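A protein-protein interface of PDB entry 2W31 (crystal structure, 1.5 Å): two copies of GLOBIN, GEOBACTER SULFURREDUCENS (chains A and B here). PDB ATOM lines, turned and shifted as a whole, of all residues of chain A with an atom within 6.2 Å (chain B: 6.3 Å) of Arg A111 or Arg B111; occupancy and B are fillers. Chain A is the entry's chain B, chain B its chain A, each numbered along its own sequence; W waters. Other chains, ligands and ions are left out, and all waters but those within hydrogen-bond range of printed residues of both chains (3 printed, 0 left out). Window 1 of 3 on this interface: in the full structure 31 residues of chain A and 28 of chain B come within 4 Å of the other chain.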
ATOM      1  N   ALA A 106      -4.143 -21.991  25.835  1.00  0.00           N
ATOM      2  CA  ALA A 106      -4.888 -20.876  26.457  1.00  0.00           C
ATOM      3  C   ALA A 106      -6.340 -20.857  25.959  1.00  0.00           C
ATOM      4  O   ALA A 106      -7.280 -20.565  26.755  1.00  0.00           O
ATOM      5  CB  ALA A 106      -4.197 -19.542  26.166  1.00  0.00           C
ATOM      6  N   MET A 107      -6.577 -21.179  24.677  1.00  0.00           N
ATOM      7  CA  MET A 107      -7.966 -21.136  24.215  1.00  0.00           C
ATOM      8  C   MET A 107      -8.784 -22.248  24.930  1.00  0.00           C
ATOM      9  O   MET A 107      -9.966 -22.044  25.236  1.00  0.00           O
ATOM     10  CB  MET A 107      -8.078 -21.278  22.695  1.00  0.00           C
ATOM     11  CG  MET A 107      -9.466 -20.899  22.173  1.00  0.00           C
ATOM     12  SD  MET A 107      -9.877 -19.147  22.435  1.00  0.00           S
ATOM     13  CE  MET A 107      -8.858 -18.348  21.223  1.00  0.00           C
ATOM     14  N   ASN A 108      -8.156 -23.398  25.242  1.00  0.00           N
ATOM     15  CA  ASN A 108      -8.883 -24.427  25.998  1.00  0.00           C
ATOM     16  C   ASN A 108      -9.277 -23.878  27.389  1.00  0.00           C
ATOM     17  O   ASN A 108     -10.400 -24.133  27.864  1.00  0.00           O
ATOM     18  CB  ASN A 108      -8.022 -25.694  26.148  1.00  0.00           C
ATOM     19  CG  ASN A 108      -8.772 -26.831  26.867  1.00  0.00           C
ATOM     20  OD1 ASN A 108      -8.571 -27.035  28.078  1.00  0.00           O
ATOM     21  ND2 ASN A 108      -9.668 -27.517  26.150  1.00  0.00           N
ATOM     22  N   VAL A 109      -8.382 -23.131  28.035  1.00  0.00           N
ATOM     23  CA  VAL A 109      -8.695 -22.515  29.354  1.00  0.00           C
ATOM     24  C   VAL A 109      -9.917 -21.600  29.249  1.00  0.00           C
ATOM     25  O   VAL A 109     -10.892 -21.695  30.062  1.00  0.00           O
ATOM     26  CB  VAL A 109      -7.487 -21.705  29.929  1.00  0.00           C
ATOM     27  CG1 VAL A 109      -7.851 -20.986  31.236  1.00  0.00           C
ATOM     28  CG2 VAL A 109      -6.339 -22.664  30.170  1.00  0.00           C
ATOM     29  N   VAL A 110      -9.917 -20.738  28.236  1.00  0.00           N
ATOM     30  CA  VAL A 110     -11.039 -19.802  28.077  1.00  0.00           C
ATOM     31  C   VAL A 110     -12.332 -20.547  27.727  1.00  0.00           C
ATOM     32  O   VAL A 110     -13.433 -20.193  28.210  1.00  0.00           O
ATOM     33  CB  VAL A 110     -10.731 -18.770  26.958  1.00  0.00           C
ATOM     34  CG1 VAL A 110     -11.950 -17.898  26.669  1.00  0.00           C
ATOM     35  CG2 VAL A 110      -9.491 -17.973  27.342  1.00  0.00           C
ATOM     36  N   ARG A 111     -12.216 -21.566  26.866  1.00  0.00           N
ATOM     37  CA  ARG A 111     -13.366 -22.356  26.468  1.00  0.00           C
ATOM     38  C   ARG A 111     -14.020 -23.021  27.668  1.00  0.00           C
ATOM     39  O   ARG A 111     -15.252 -22.960  27.839  1.00  0.00           O
ATOM     40  CB  ARG A 111     -12.912 -23.411  25.447  1.00  0.00           C
ATOM     41  CG  ARG A 111     -14.019 -24.192  24.809  1.00  0.00           C
ATOM     42  CD  ARG A 111     -13.450 -25.407  23.969  1.00  0.00           C
ATOM     43  NE  ARG A 111     -12.299 -25.086  23.088  1.00  0.00           N
ATOM     44  CZ  ARG A 111     -12.435 -24.523  21.877  1.00  0.00           C
ATOM     45  NH1 ARG A 111     -13.635 -24.111  21.483  1.00  0.00           N
ATOM     46  NH2 ARG A 111     -11.371 -24.331  21.077  1.00  0.00           N
ATOM     47  N   GLN A 112     -13.210 -23.667  28.512  1.00  0.00           N
ATOM     48  CA  GLN A 112     -13.786 -24.364  29.674  1.00  0.00           C
ATOM     49  C   GLN A 112     -14.475 -23.355  30.613  1.00  0.00           C
ATOM     50  O   GLN A 112     -15.559 -23.599  31.154  1.00  0.00           O
ATOM     51  CB  GLN A 112     -12.696 -25.133  30.448  1.00  0.00           C
ATOM     52  CG  GLN A 112     -11.851 -26.165  29.646  1.00  0.00           C
ATOM     53  CD  GLN A 112     -12.537 -27.485  29.294  1.00  0.00           C
ATOM     54  OE1 GLN A 112     -13.777 -27.578  29.276  1.00  0.00           O
ATOM     55  NE2 GLN A 112     -11.714 -28.530  28.970  1.00  0.00           N
ATOM     56  N   PHE A 113     -13.813 -22.224  30.835  1.00  0.00           N
ATOM     57  CA  PHE A 113     -14.380 -21.191  31.710  1.00  0.00           C
ATOM     58  C   PHE A 113     -15.719 -20.672  31.201  1.00  0.00           C
ATOM     59  O   PHE A 113     -16.711 -20.517  31.979  1.00  0.00           O
ATOM     60  CB  PHE A 113     -13.363 -20.067  31.862  1.00  0.00           C
ATOM     61  CG  PHE A 113     -13.810 -18.955  32.762  1.00  0.00           C
ATOM     62  CD1 PHE A 113     -13.345 -18.891  34.084  1.00  0.00           C
ATOM     63  CD2 PHE A 113     -14.642 -17.951  32.286  1.00  0.00           C
ATOM     64  CE1 PHE A 113     -13.764 -17.819  34.937  1.00  0.00           C
ATOM     65  CE2 PHE A 113     -15.044 -16.866  33.098  1.00  0.00           C
ATOM     66  CZ  PHE A 113     -14.619 -16.821  34.415  1.00  0.00           C
ATOM     67  N   THR A 114     -15.778 -20.411  29.885  1.00  0.00           N
ATOM     68  CA  THR A 114     -16.955 -19.784  29.305  1.00  0.00           C
ATOM     69  C   THR A 114     -18.096 -20.785  29.246  1.00  0.00           C
ATOM     70  O   THR A 114     -19.263 -20.417  29.506  1.00  0.00           O
ATOM     71  CB  THR A 114     -16.643 -19.192  27.901  1.00  0.00           C
ATOM     72  OG1 THR A 114     -15.518 -18.316  28.015  1.00  0.00           O
ATOM     73  CG2 THR A 114     -17.821 -18.387  27.355  1.00  0.00           C
ATOM     74  N   LEU A 115     -17.803 -22.039  28.872  1.00  0.00           N
ATOM     75  CA  LEU A 115     -18.880 -23.034  28.855  1.00  0.00           C
ATOM     76  C   LEU A 115     -19.436 -23.312  30.269  1.00  0.00           C
ATOM     77  O   LEU A 115     -20.623 -23.674  30.423  1.00  0.00           O
ATOM     78  CB  LEU A 115     -18.444 -24.319  28.123  1.00  0.00           C
ATOM     79  CG  LEU A 115     -18.161 -24.143  26.626  1.00  0.00           C
ATOM     80  CD1 LEU A 115     -18.209 -25.518  26.026  1.00  0.00           C
ATOM     81  CD2 LEU A 115     -19.033 -23.219  25.838  1.00  0.00           C
ATOM     82  N   SER A 116     -18.596 -23.145  31.296  1.00  0.00           N
ATOM     83  CA  SER A 116     -19.121 -23.235  32.688  1.00  0.00           C
ATOM     84  C   SER A 116     -20.042 -22.062  33.031  1.00  0.00           C
ATOM     85  O   SER A 116     -21.035 -22.256  33.733  1.00  0.00           O
ATOM     86  CB  SER A 116     -17.983 -23.389  33.700  1.00  0.00           C
ATOM     87  OG  SER A 116     -17.555 -24.751  33.688  1.00  0.00           O
ATOM     88  N   ARG A 132     -24.076 -22.108  23.911  1.00  0.00           N
ATOM     89  CA  ARG A 132     -22.872 -22.917  23.748  1.00  0.00           C
ATOM     90  C   ARG A 132     -22.415 -22.952  22.286  1.00  0.00           C
ATOM     91  O   ARG A 132     -21.211 -22.820  21.994  1.00  0.00           O
ATOM     92  CB  ARG A 132     -23.105 -24.353  24.261  1.00  0.00           C
ATOM     93  CG  ARG A 132     -21.887 -25.262  24.039  1.00  0.00           C
ATOM     94  CD  ARG A 132     -22.019 -26.178  22.861  1.00  0.00           C
ATOM     95  NE  ARG A 132     -23.107 -27.135  23.064  1.00  0.00           N
ATOM     96  CZ  ARG A 132     -23.613 -27.922  22.125  1.00  0.00           C
ATOM     97  NH1 ARG A 132     -23.132 -27.897  20.884  1.00  0.00           N
ATOM     98  NH2 ARG A 132     -24.602 -28.746  22.437  1.00  0.00           N
ATOM     99  N   VAL A 135     -20.883 -19.590  21.293  1.00  0.00           N
ATOM    100  CA  VAL A 135     -19.576 -19.419  21.964  1.00  0.00           C
ATOM    101  C   VAL A 135     -18.496 -20.322  21.306  1.00  0.00           C
ATOM    102  O   VAL A 135     -17.346 -19.864  21.041  1.00  0.00           O
ATOM    103  CB  VAL A 135     -19.659 -19.700  23.486  1.00  0.00           C
ATOM    104  CG1 VAL A 135     -18.257 -19.900  24.092  1.00  0.00           C
ATOM    105  CG2 VAL A 135     -20.409 -18.580  24.219  1.00  0.00           C
ATOM    106  N   GLU A 136     -18.839 -21.583  21.045  1.00  0.00           N
ATOM    107  CA  GLU A 136     -17.826 -22.472  20.464  1.00  0.00           C
ATOM    108  C   GLU A 136     -17.405 -21.930  19.074  1.00  0.00           C
ATOM    109  O   GLU A 136     -16.223 -22.028  18.701  1.00  0.00           O
ATOM    110  CB  GLU A 136     -18.375 -23.894  20.304  1.00  0.00           C
ATOM    111  CG  GLU A 136     -18.622 -24.577  21.658  1.00  0.00           C
ATOM    112  CD  GLU A 136     -17.382 -25.151  22.313  1.00  0.00           C
ATOM    113  OE1 GLU A 136     -16.353 -24.487  22.439  1.00  0.00           O
ATOM    114  OE2 GLU A 136     -17.481 -26.326  22.741  1.00  0.00           O
ATOM    115  N   LEU A 139     -15.057 -18.747  19.600  1.00  0.00           N
ATOM    116  CA  LEU A 139     -13.728 -19.163  20.104  1.00  0.00           C
ATOM    117  C   LEU A 139     -12.938 -19.876  19.023  1.00  0.00           C
ATOM    118  O   LEU A 139     -11.744 -19.598  18.845  1.00  0.00           O
ATOM    119  CB  LEU A 139     -13.878 -20.051  21.358  1.00  0.00           C
ATOM    120  CG  LEU A 139     -14.433 -19.346  22.597  1.00  0.00           C
ATOM    121  CD1 LEU A 139     -14.492 -20.335  23.787  1.00  0.00           C
ATOM    122  CD2 LEU A 139     -13.594 -18.090  22.953  1.00  0.00           C
ATOM    123  N   ASP A 140     -13.601 -20.790  18.289  1.00  0.00           N
ATOM    124  CA  ASP A 140     -12.919 -21.526  17.199  1.00  0.00           C
ATOM    125  C   ASP A 140     -12.475 -20.562  16.079  1.00  0.00           C
ATOM    126  O   ASP A 140     -11.390 -20.753  15.480  1.00  0.00           O
ATOM    127  CB  ASP A 140     -13.744 -22.685  16.695  1.00  0.00           C
ATOM    128  CG  ASP A 140     -13.746 -23.866  17.666  1.00  0.00           C
ATOM    129  OD1 ASP A 140     -13.042 -23.809  18.701  1.00  0.00           O
ATOM    130  OD2 ASP A 140     -14.438 -24.872  17.358  1.00  0.00           O
ATOM    131  N   LEU A 143      -9.309 -18.819  17.399  1.00  0.00           N
ATOM    132  CA  LEU A 143      -8.193 -19.747  17.320  1.00  0.00           C
ATOM    133  C   LEU A 143      -7.717 -19.944  15.877  1.00  0.00           C
ATOM    134  O   LEU A 143      -6.485 -20.012  15.637  1.00  0.00           O
ATOM    135  CB  LEU A 143      -8.583 -21.083  17.981  1.00  0.00           C
ATOM    136  CG  LEU A 143      -7.498 -22.162  18.026  1.00  0.00           C
ATOM    137  CD1 LEU A 143      -6.233 -21.666  18.761  1.00  0.00           C
ATOM    138  CD2 LEU A 143      -8.138 -23.375  18.723  1.00  0.00           C
ATOM    139  N   ASN B 104      -9.702 -26.562  11.186  1.00  0.00           N
ATOM    140  CA  ASN B 104     -10.397 -25.859  12.281  1.00  0.00           C
ATOM    141  C   ASN B 104     -11.922 -25.890  12.118  1.00  0.00           C
ATOM    142  O   ASN B 104     -12.679 -26.104  13.108  1.00  0.00           O
ATOM    143  CB  ASN B 104      -9.904 -24.419  12.416  1.00  0.00           C
ATOM    144  CG  ASN B 104      -8.438 -24.321  12.907  1.00  0.00           C
ATOM    145  OD1 ASN B 104      -8.140 -23.960  14.093  1.00  0.00           O
ATOM    146  ND2 ASN B 104      -7.522 -24.533  11.989  1.00  0.00           N
ATOM    147  N   ALA B 106     -13.752 -28.133  10.473  1.00  0.00           N
ATOM    148  CA  ALA B 106     -14.243 -29.489  10.686  1.00  0.00           C
ATOM    149  C   ALA B 106     -14.300 -29.827  12.173  1.00  0.00           C
ATOM    150  O   ALA B 106     -15.189 -30.551  12.621  1.00  0.00           O
ATOM    151  CB  ALA B 106     -13.371 -30.492   9.946  1.00  0.00           C
ATOM    152  N   MET B 107     -13.346 -29.298  12.932  1.00  0.00           N
ATOM    153  CA  MET B 107     -13.223 -29.626  14.347  1.00  0.00           C
ATOM    154  C   MET B 107     -14.328 -28.967  15.165  1.00  0.00           C
ATOM    155  O   MET B 107     -14.739 -29.486  16.203  1.00  0.00           O
ATOM    156  CB  MET B 107     -11.852 -29.203  14.877  1.00  0.00           C
ATOM    157  CG  MET B 107     -11.529 -29.740  16.263  1.00  0.00           C
ATOM    158  SD  MET B 107     -11.524 -31.542  16.326  1.00  0.00           S
ATOM    159  CE  MET B 107      -9.872 -31.897  15.731  1.00  0.00           C
ATOM    160  N   ASN B 108     -14.804 -27.820  14.691  1.00  0.00           N
ATOM    161  CA  ASN B 108     -16.011 -27.187  15.261  1.00  0.00           C
ATOM    162  C   ASN B 108     -17.257 -28.083  15.059  1.00  0.00           C
ATOM    163  O   ASN B 108     -18.086 -28.228  15.993  1.00  0.00           O
ATOM    164  CB  ASN B 108     -16.243 -25.784  14.667  1.00  0.00           C
ATOM    165  CG  ASN B 108     -17.386 -25.058  15.372  1.00  0.00           C
ATOM    166  OD1 ASN B 108     -18.521 -25.079  14.889  1.00  0.00           O
ATOM    167  ND2 ASN B 108     -17.120 -24.523  16.567  1.00  0.00           N
ATOM    168  N   VAL B 109     -17.372 -28.687  13.860  1.00  0.00           N
ATOM    169  CA  VAL B 109     -18.490 -29.588  13.604  1.00  0.00           C
ATOM    170  C   VAL B 109     -18.496 -30.760  14.623  1.00  0.00           C
ATOM    171  O   VAL B 109     -19.525 -31.109  15.204  1.00  0.00           O
ATOM    172  CB  VAL B 109     -18.448 -30.143  12.161  1.00  0.00           C
ATOM    173  CG1 VAL B 109     -19.632 -31.144  11.932  1.00  0.00           C
ATOM    174  CG2 VAL B 109     -18.481 -28.998  11.160  1.00  0.00           C
ATOM    175  N   VAL B 110     -17.336 -31.391  14.802  1.00  0.00           N
ATOM    176  CA  VAL B 110     -17.228 -32.516  15.742  1.00  0.00           C
ATOM    177  C   VAL B 110     -17.527 -32.054  17.178  1.00  0.00           C
ATOM    178  O   VAL B 110     -18.202 -32.744  17.965  1.00  0.00           O
ATOM    179  CB  VAL B 110     -15.828 -33.152  15.631  1.00  0.00           C
ATOM    180  CG1 VAL B 110     -15.625 -34.279  16.622  1.00  0.00           C
ATOM    181  CG2 VAL B 110     -15.585 -33.636  14.195  1.00  0.00           C
ATOM    182  N   ARG B 111     -17.007 -30.883  17.522  1.00  0.00           N
ATOM    183  CA  ARG B 111     -17.175 -30.379  18.879  1.00  0.00           C
ATOM    184  C   ARG B 111     -18.677 -30.148  19.187  1.00  0.00           C
ATOM    185  O   ARG B 111     -19.177 -30.553  20.225  1.00  0.00           O
ATOM    186  CB  ARG B 111     -16.403 -29.067  18.965  1.00  0.00           C
ATOM    187  CG  ARG B 111     -16.263 -28.541  20.293  1.00  0.00           C
ATOM    188  CD  ARG B 111     -15.714 -27.080  20.179  1.00  0.00           C
ATOM    189  NE  ARG B 111     -14.466 -26.903  19.419  1.00  0.00           N
ATOM    190  CZ  ARG B 111     -13.252 -27.253  19.884  1.00  0.00           C
ATOM    191  NH1 ARG B 111     -13.133 -27.871  21.040  1.00  0.00           N
ATOM    192  NH2 ARG B 111     -12.141 -27.045  19.192  1.00  0.00           N
ATOM    193  N   GLN B 112     -19.421 -29.529  18.259  1.00  0.00           N
ATOM    194  CA  GLN B 112     -20.829 -29.198  18.536  1.00  0.00           C
ATOM    195  C   GLN B 112     -21.601 -30.511  18.637  1.00  0.00           C
ATOM    196  O   GLN B 112     -22.470 -30.660  19.501  1.00  0.00           O
ATOM    197  CB  GLN B 112     -21.399 -28.333  17.404  1.00  0.00           C
ATOM    198  CG  GLN B 112     -20.570 -27.058  17.114  1.00  0.00           C
ATOM    199  CD  GLN B 112     -20.884 -25.872  18.025  1.00  0.00           C
ATOM    200  OE1 GLN B 112     -21.341 -26.047  19.169  1.00  0.00           O
ATOM    201  NE2 GLN B 112     -20.614 -24.646  17.524  1.00  0.00           N
ATOM    202  N   PHE B 113     -21.271 -31.469  17.761  1.00  0.00           N
ATOM    203  CA  PHE B 113     -21.999 -32.741  17.732  1.00  0.00           C
ATOM    204  C   PHE B 113     -21.797 -33.489  19.054  1.00  0.00           C
ATOM    205  O   PHE B 113     -22.768 -34.024  19.658  1.00  0.00           O
ATOM    206  CB  PHE B 113     -21.460 -33.591  16.581  1.00  0.00           C
ATOM    207  CG  PHE B 113     -22.156 -34.950  16.424  1.00  0.00           C
ATOM    208  CD1 PHE B 113     -23.291 -35.106  15.609  1.00  0.00           C
ATOM    209  CD2 PHE B 113     -21.664 -36.066  17.107  1.00  0.00           C
ATOM    210  CE1 PHE B 113     -23.926 -36.350  15.494  1.00  0.00           C
ATOM    211  CE2 PHE B 113     -22.287 -37.336  16.970  1.00  0.00           C
ATOM    212  CZ  PHE B 113     -23.417 -37.456  16.188  1.00  0.00           C
ATOM    213  N   THR B 114     -20.538 -33.563  19.505  1.00  0.00           N
ATOM    214  CA  THR B 114     -20.214 -34.339  20.708  1.00  0.00           C
ATOM    215  C   THR B 114     -20.752 -33.688  21.969  1.00  0.00           C
ATOM    216  O   THR B 114     -21.271 -34.387  22.863  1.00  0.00           O
ATOM    217  CB  THR B 114     -18.708 -34.547  20.787  1.00  0.00           C
ATOM    218  OG1 THR B 114     -18.272 -35.116  19.550  1.00  0.00           O
ATOM    219  CG2 THR B 114     -18.353 -35.535  21.903  1.00  0.00           C
ATOM    220  N   LEU B 115     -20.741 -32.356  22.030  1.00  0.00           N
ATOM    221  CA  LEU B 115     -21.287 -31.715  23.214  1.00  0.00           C
ATOM    222  C   LEU B 115     -22.807 -31.862  23.274  1.00  0.00           C
ATOM    223  O   LEU B 115     -23.390 -31.861  24.405  1.00  0.00           O
ATOM    224  CB  LEU B 115     -20.845 -30.243  23.350  1.00  0.00           C
ATOM    225  CG  LEU B 115     -19.350 -30.074  23.599  1.00  0.00           C
ATOM    226  CD1 LEU B 115     -19.113 -28.634  24.155  1.00  0.00           C
ATOM    227  CD2 LEU B 115     -18.575 -31.091  24.394  1.00  0.00           C
ATOM    228  N   SER B 116     -23.440 -31.945  22.109  1.00  0.00           N
ATOM    229  CA  SER B 116     -24.887 -32.212  22.109  1.00  0.00           C
ATOM    230  C   SER B 116     -25.194 -33.612  22.624  1.00  0.00           C
ATOM    231  O   SER B 116     -26.167 -33.780  23.382  1.00  0.00           O
ATOM    232  CB  SER B 116     -25.514 -31.928  20.755  1.00  0.00           C
ATOM    233  OG  SER B 116     -25.738 -30.524  20.714  1.00  0.00           O
ATOM    234  N   ARG B 132     -17.865 -33.014  29.495  1.00  0.00           N
ATOM    235  CA  ARG B 132     -17.592 -31.935  28.553  1.00  0.00           C
ATOM    236  C   ARG B 132     -16.125 -31.508  28.666  1.00  0.00           C
ATOM    237  O   ARG B 132     -15.462 -31.276  27.623  1.00  0.00           O
ATOM    238  CB  ARG B 132     -18.528 -30.741  28.794  1.00  0.00           C
ATOM    239  CG  ARG B 132     -18.492 -29.700  27.670  1.00  0.00           C
ATOM    240  CD  ARG B 132     -19.342 -28.481  27.977  1.00  0.00           C
ATOM    241  NE  ARG B 132     -18.945 -27.819  29.228  1.00  0.00           N
ATOM    242  CZ  ARG B 132     -19.713 -27.714  30.314  1.00  0.00           C
ATOM    243  NH1 ARG B 132     -20.937 -28.210  30.329  1.00  0.00           N
ATOM    244  NH2 ARG B 132     -19.248 -27.098  31.393  1.00  0.00           N
ATOM    245  N   VAL B 135     -13.839 -34.074  26.887  1.00  0.00           N
ATOM    246  CA  VAL B 135     -13.995 -34.040  25.418  1.00  0.00           C
ATOM    247  C   VAL B 135     -13.343 -32.768  24.859  1.00  0.00           C
ATOM    248  O   VAL B 135     -12.632 -32.822  23.842  1.00  0.00           O
ATOM    249  CB  VAL B 135     -15.480 -34.078  25.017  1.00  0.00           C
ATOM    250  CG1 VAL B 135     -15.693 -33.600  23.583  1.00  0.00           C
ATOM    251  CG2 VAL B 135     -16.020 -35.490  25.240  1.00  0.00           C
ATOM    252  N   GLU B 136     -13.564 -31.624  25.514  1.00  0.00           N
ATOM    253  CA  GLU B 136     -12.901 -30.401  25.001  1.00  0.00           C
ATOM    254  C   GLU B 136     -11.383 -30.506  25.015  1.00  0.00           C
ATOM    255  O   GLU B 136     -10.721 -30.029  24.073  1.00  0.00           O
ATOM    256  CB  GLU B 136     -13.356 -29.155  25.739  1.00  0.00           C
ATOM    257  CG  GLU B 136     -14.832 -28.837  25.605  1.00  0.00           C
ATOM    258  CD  GLU B 136     -15.219 -28.110  24.363  1.00  0.00           C
ATOM    259  OE1 GLU B 136     -14.780 -28.438  23.242  1.00  0.00           O
ATOM    260  OE2 GLU B 136     -16.081 -27.198  24.498  1.00  0.00           O
ATOM    261  N   LEU B 139     -10.320 -32.989  22.030  1.00  0.00           N
ATOM    262  CA  LEU B 139     -10.521 -32.333  20.702  1.00  0.00           C
ATOM    263  C   LEU B 139      -9.460 -31.239  20.528  1.00  0.00           C
ATOM    264  O   LEU B 139      -8.862 -31.109  19.445  1.00  0.00           O
ATOM    265  CB  LEU B 139     -11.928 -31.724  20.556  1.00  0.00           C
ATOM    266  CG  LEU B 139     -13.042 -32.764  20.586  1.00  0.00           C
ATOM    267  CD1 LEU B 139     -14.370 -32.041  20.522  1.00  0.00           C
ATOM    268  CD2 LEU B 139     -12.888 -33.698  19.428  1.00  0.00           C
ATOM    269  N   ASP B 140      -9.244 -30.425  21.573  1.00  0.00           N
ATOM    270  CA  ASP B 140      -8.237 -29.332  21.472  1.00  0.00           C
ATOM    271  C   ASP B 140      -6.819 -29.876  21.288  1.00  0.00           C
ATOM    272  O   ASP B 140      -6.036 -29.286  20.534  1.00  0.00           O
ATOM    273  CB  ASP B 140      -8.357 -28.348  22.650  1.00  0.00           C
ATOM    274  CG  ASP B 140      -9.550 -27.398  22.506  1.00  0.00           C
ATOM    275  OD1 ASP B 140     -10.273 -27.461  21.473  1.00  0.00           O
ATOM    276  OD2 ASP B 140      -9.756 -26.605  23.453  1.00  0.00           O
ATOM    277  N   LEU B 143      -6.608 -30.940  17.582  1.00  0.00           N
ATOM    278  CA  LEU B 143      -6.483 -29.774  16.716  1.00  0.00           C
ATOM    279  C   LEU B 143      -5.090 -29.125  16.847  1.00  0.00           C
ATOM    280  O   LEU B 143      -4.491 -28.673  15.850  1.00  0.00           O
ATOM    281  CB  LEU B 143      -7.582 -28.756  17.111  1.00  0.00           C
ATOM    282  CG  LEU B 143      -7.600 -27.448  16.306  1.00  0.00           C
ATOM    283  CD1 LEU B 143      -7.780 -27.685  14.803  1.00  0.00           C
ATOM    284  CD2 LEU B 143      -8.720 -26.545  16.844  1.00  0.00           C
HETATM  285  O   HOH W   1     -10.375 -23.406  15.788  1.00  0.00           O
HETATM  286  O   HOH W   2     -24.782 -28.741  18.662  1.00  0.00           O
HETATM  287  O   HOH W   3     -12.163 -25.650  15.790  1.00  0.00           O
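ND2 of Asn B108 is in hydrogen-bond range of O of Glu A136, at 3.4 Å.
The side-chain amide oxygen (OE1) of Gln B112 sits at hydrogen-bond distance from the guanidinium group (NH1) of Arg A132, 3.1 Å away.
The side-chain carboxylate (OE2) of Glu A136 lies close to the side-chain carboxylate (OE2) of Glu B136 (2.4 Å).
The guanidinium group of Arg B111 lies within salt-bridge range of the side-chain carboxylate of Asp A140 (2.9 Å).
NH2 of Arg B111 lies close to NH2 of Arg A111, 3.4 Å away.
The side-chain carboxylate (OD2) of Asp B140 is in salt-bridge range of the guanidinium group (NE) of Arg A111 (3.0 Å).
The backbone carbonyl oxygen (O) of Glu B136 is in hydrogen-bond range of the side-chain amide nitrogen (ND2) of Asn A108 (3.4 Å).
ND2 of Asn B108 sits at hydrogen-bond distance from OD2 of Asp A140, at 2.8 Å.
The side-chain hydroxyl of Ser B116 sits at hydrogen-bond distance from the guanidinium group of Arg A132 (2.7 Å).
The side-chain carboxylate of Asp B140 lies within hydrogen-bond range of the side-chain amide nitrogen of Asn A108, 2.8 Å away.
NH1 of Arg A111 lies within salt-bridge range of OE1 of Glu A136 (2.9 Å).
The guanidinium group of Arg B111 is in salt-bridge range of the side-chain carboxylate of Asp B140.
The side-chain amide nitrogen of Gln B112 lies within hydrogen-bond range of the side-chain amide oxygen of Asn B108, at 3.4 Å.
NH1 of Arg A111 lies within salt-bridge range of OD1 of Asp A140 (2.9 Å).
The backbone carbonyl oxygen of Gln A112 sits at hydrogen-bond distance from the side-chain hydroxyl of Ser A116 (3.4 Å).
The guanidinium group (NH1) of Arg B111 is in salt-bridge range of the side-chain carboxylate (OE1) of Glu B136 (2.8 Å).
Among the printed residues, pairs that only touch across the chains: Arg A111 with Glu B136 (3.2 Å), Gln A112 with Glu B136 (3.7 Å), Leu A115 with Leu B115 (3.7 Å), Leu A115 with Arg B132 (3.7 Å), Leu A115 with Glu B136 (3.1 Å), Ser A116 with Arg B132 (3.7 Å), Arg A132 with Leu B115 (3.7 Å), Glu A136 with Arg B111 (3.2 Å), Glu A136 with Gln B112 (3.6 Å), Glu A136 with Leu B115 (3.2 Å) and Leu A143 with Leu B143 (3.7 Å).
Arg A111 touches just these residues of chain B: Arg B111, Glu B136 and Asp B140.
Of the printed residues of chain B, Gln A112 touches Glu B136 (3.7 Å).
Of the printed residues of chain B, Ser A116 touches Arg B132.
Of the printed residues of chain A, Asn B108 touches Glu A136 (3.4 Å) and Asp A140 (2.8 Å).
Val B110 touches none of the printed residues of chain A.
Of chain A, only Arg A111 (3.4 Å), Glu A136 (3.2 Å) and Asp A140 (2.9 Å) come within 4 Å of Arg B111.
Of the printed residues of chain A, Gln B112 touches Arg A132 (3.1 Å) and Glu A136 (3.6 Å).
Printed residues of chain A within 4 Å of Leu B143: Leu A143.
The nearest printed residue of chain B that does not touch Arg A111 is Leu B143 (5.5 Å).
The nearest printed residue of chain B that does not touch Ser A116 is Glu B136 (8.3 Å).
Of the 18 printed residues of chain B, 9 touch a printed residue of chain A.
Printed residues of chain B that touch a printed residue of chain A: Asn B108, Arg B111, Gln B112, Leu B115, Ser B116, Arg B132, Glu B136, Asp B140 and Leu B143.
Hydrophobic or aromatic side chains of chain B within 4 Å of the printed part of chain A: Leu B115 and Leu B143.
Among the printed residues, 21 pairs touch across the chains.
Among the printed residues, Asp or Glu carboxylates within 4 Å of a Lys or Arg side-chain nitrogen of the other chain: Arg A111 with Asp B140 and Asp A140 with Arg B111.
Asn A108 touches Glu B136, and with the chains exchanged Glu A136 touches Asn B108.
Arg A111 touches its own counterpart, Arg B111.
Gln A112 touches Glu B136, and with the chains exchanged Glu A136 touches Gln B112.
Leu B115 touches its own counterpart, Leu A115.
17 positions are printed for both chains.
Water W3 lies within hydrogen-bond range of the backbone carbonyl oxygen (O) of Asn B104 (2.8 Å) and the side-chain carboxylate (OD2) of Asp A140 (2.9 Å).
Water W1 lies within hydrogen-bond range of the backbone carbonyl oxygen of Asp A140 (2.9 Å) and the side-chain amide oxygen of Asn B104 (2.9 Å).
Water W2 lies within hydrogen-bond range of OG of Ser B116, NH1 of Arg A132 and O of Gln B112.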
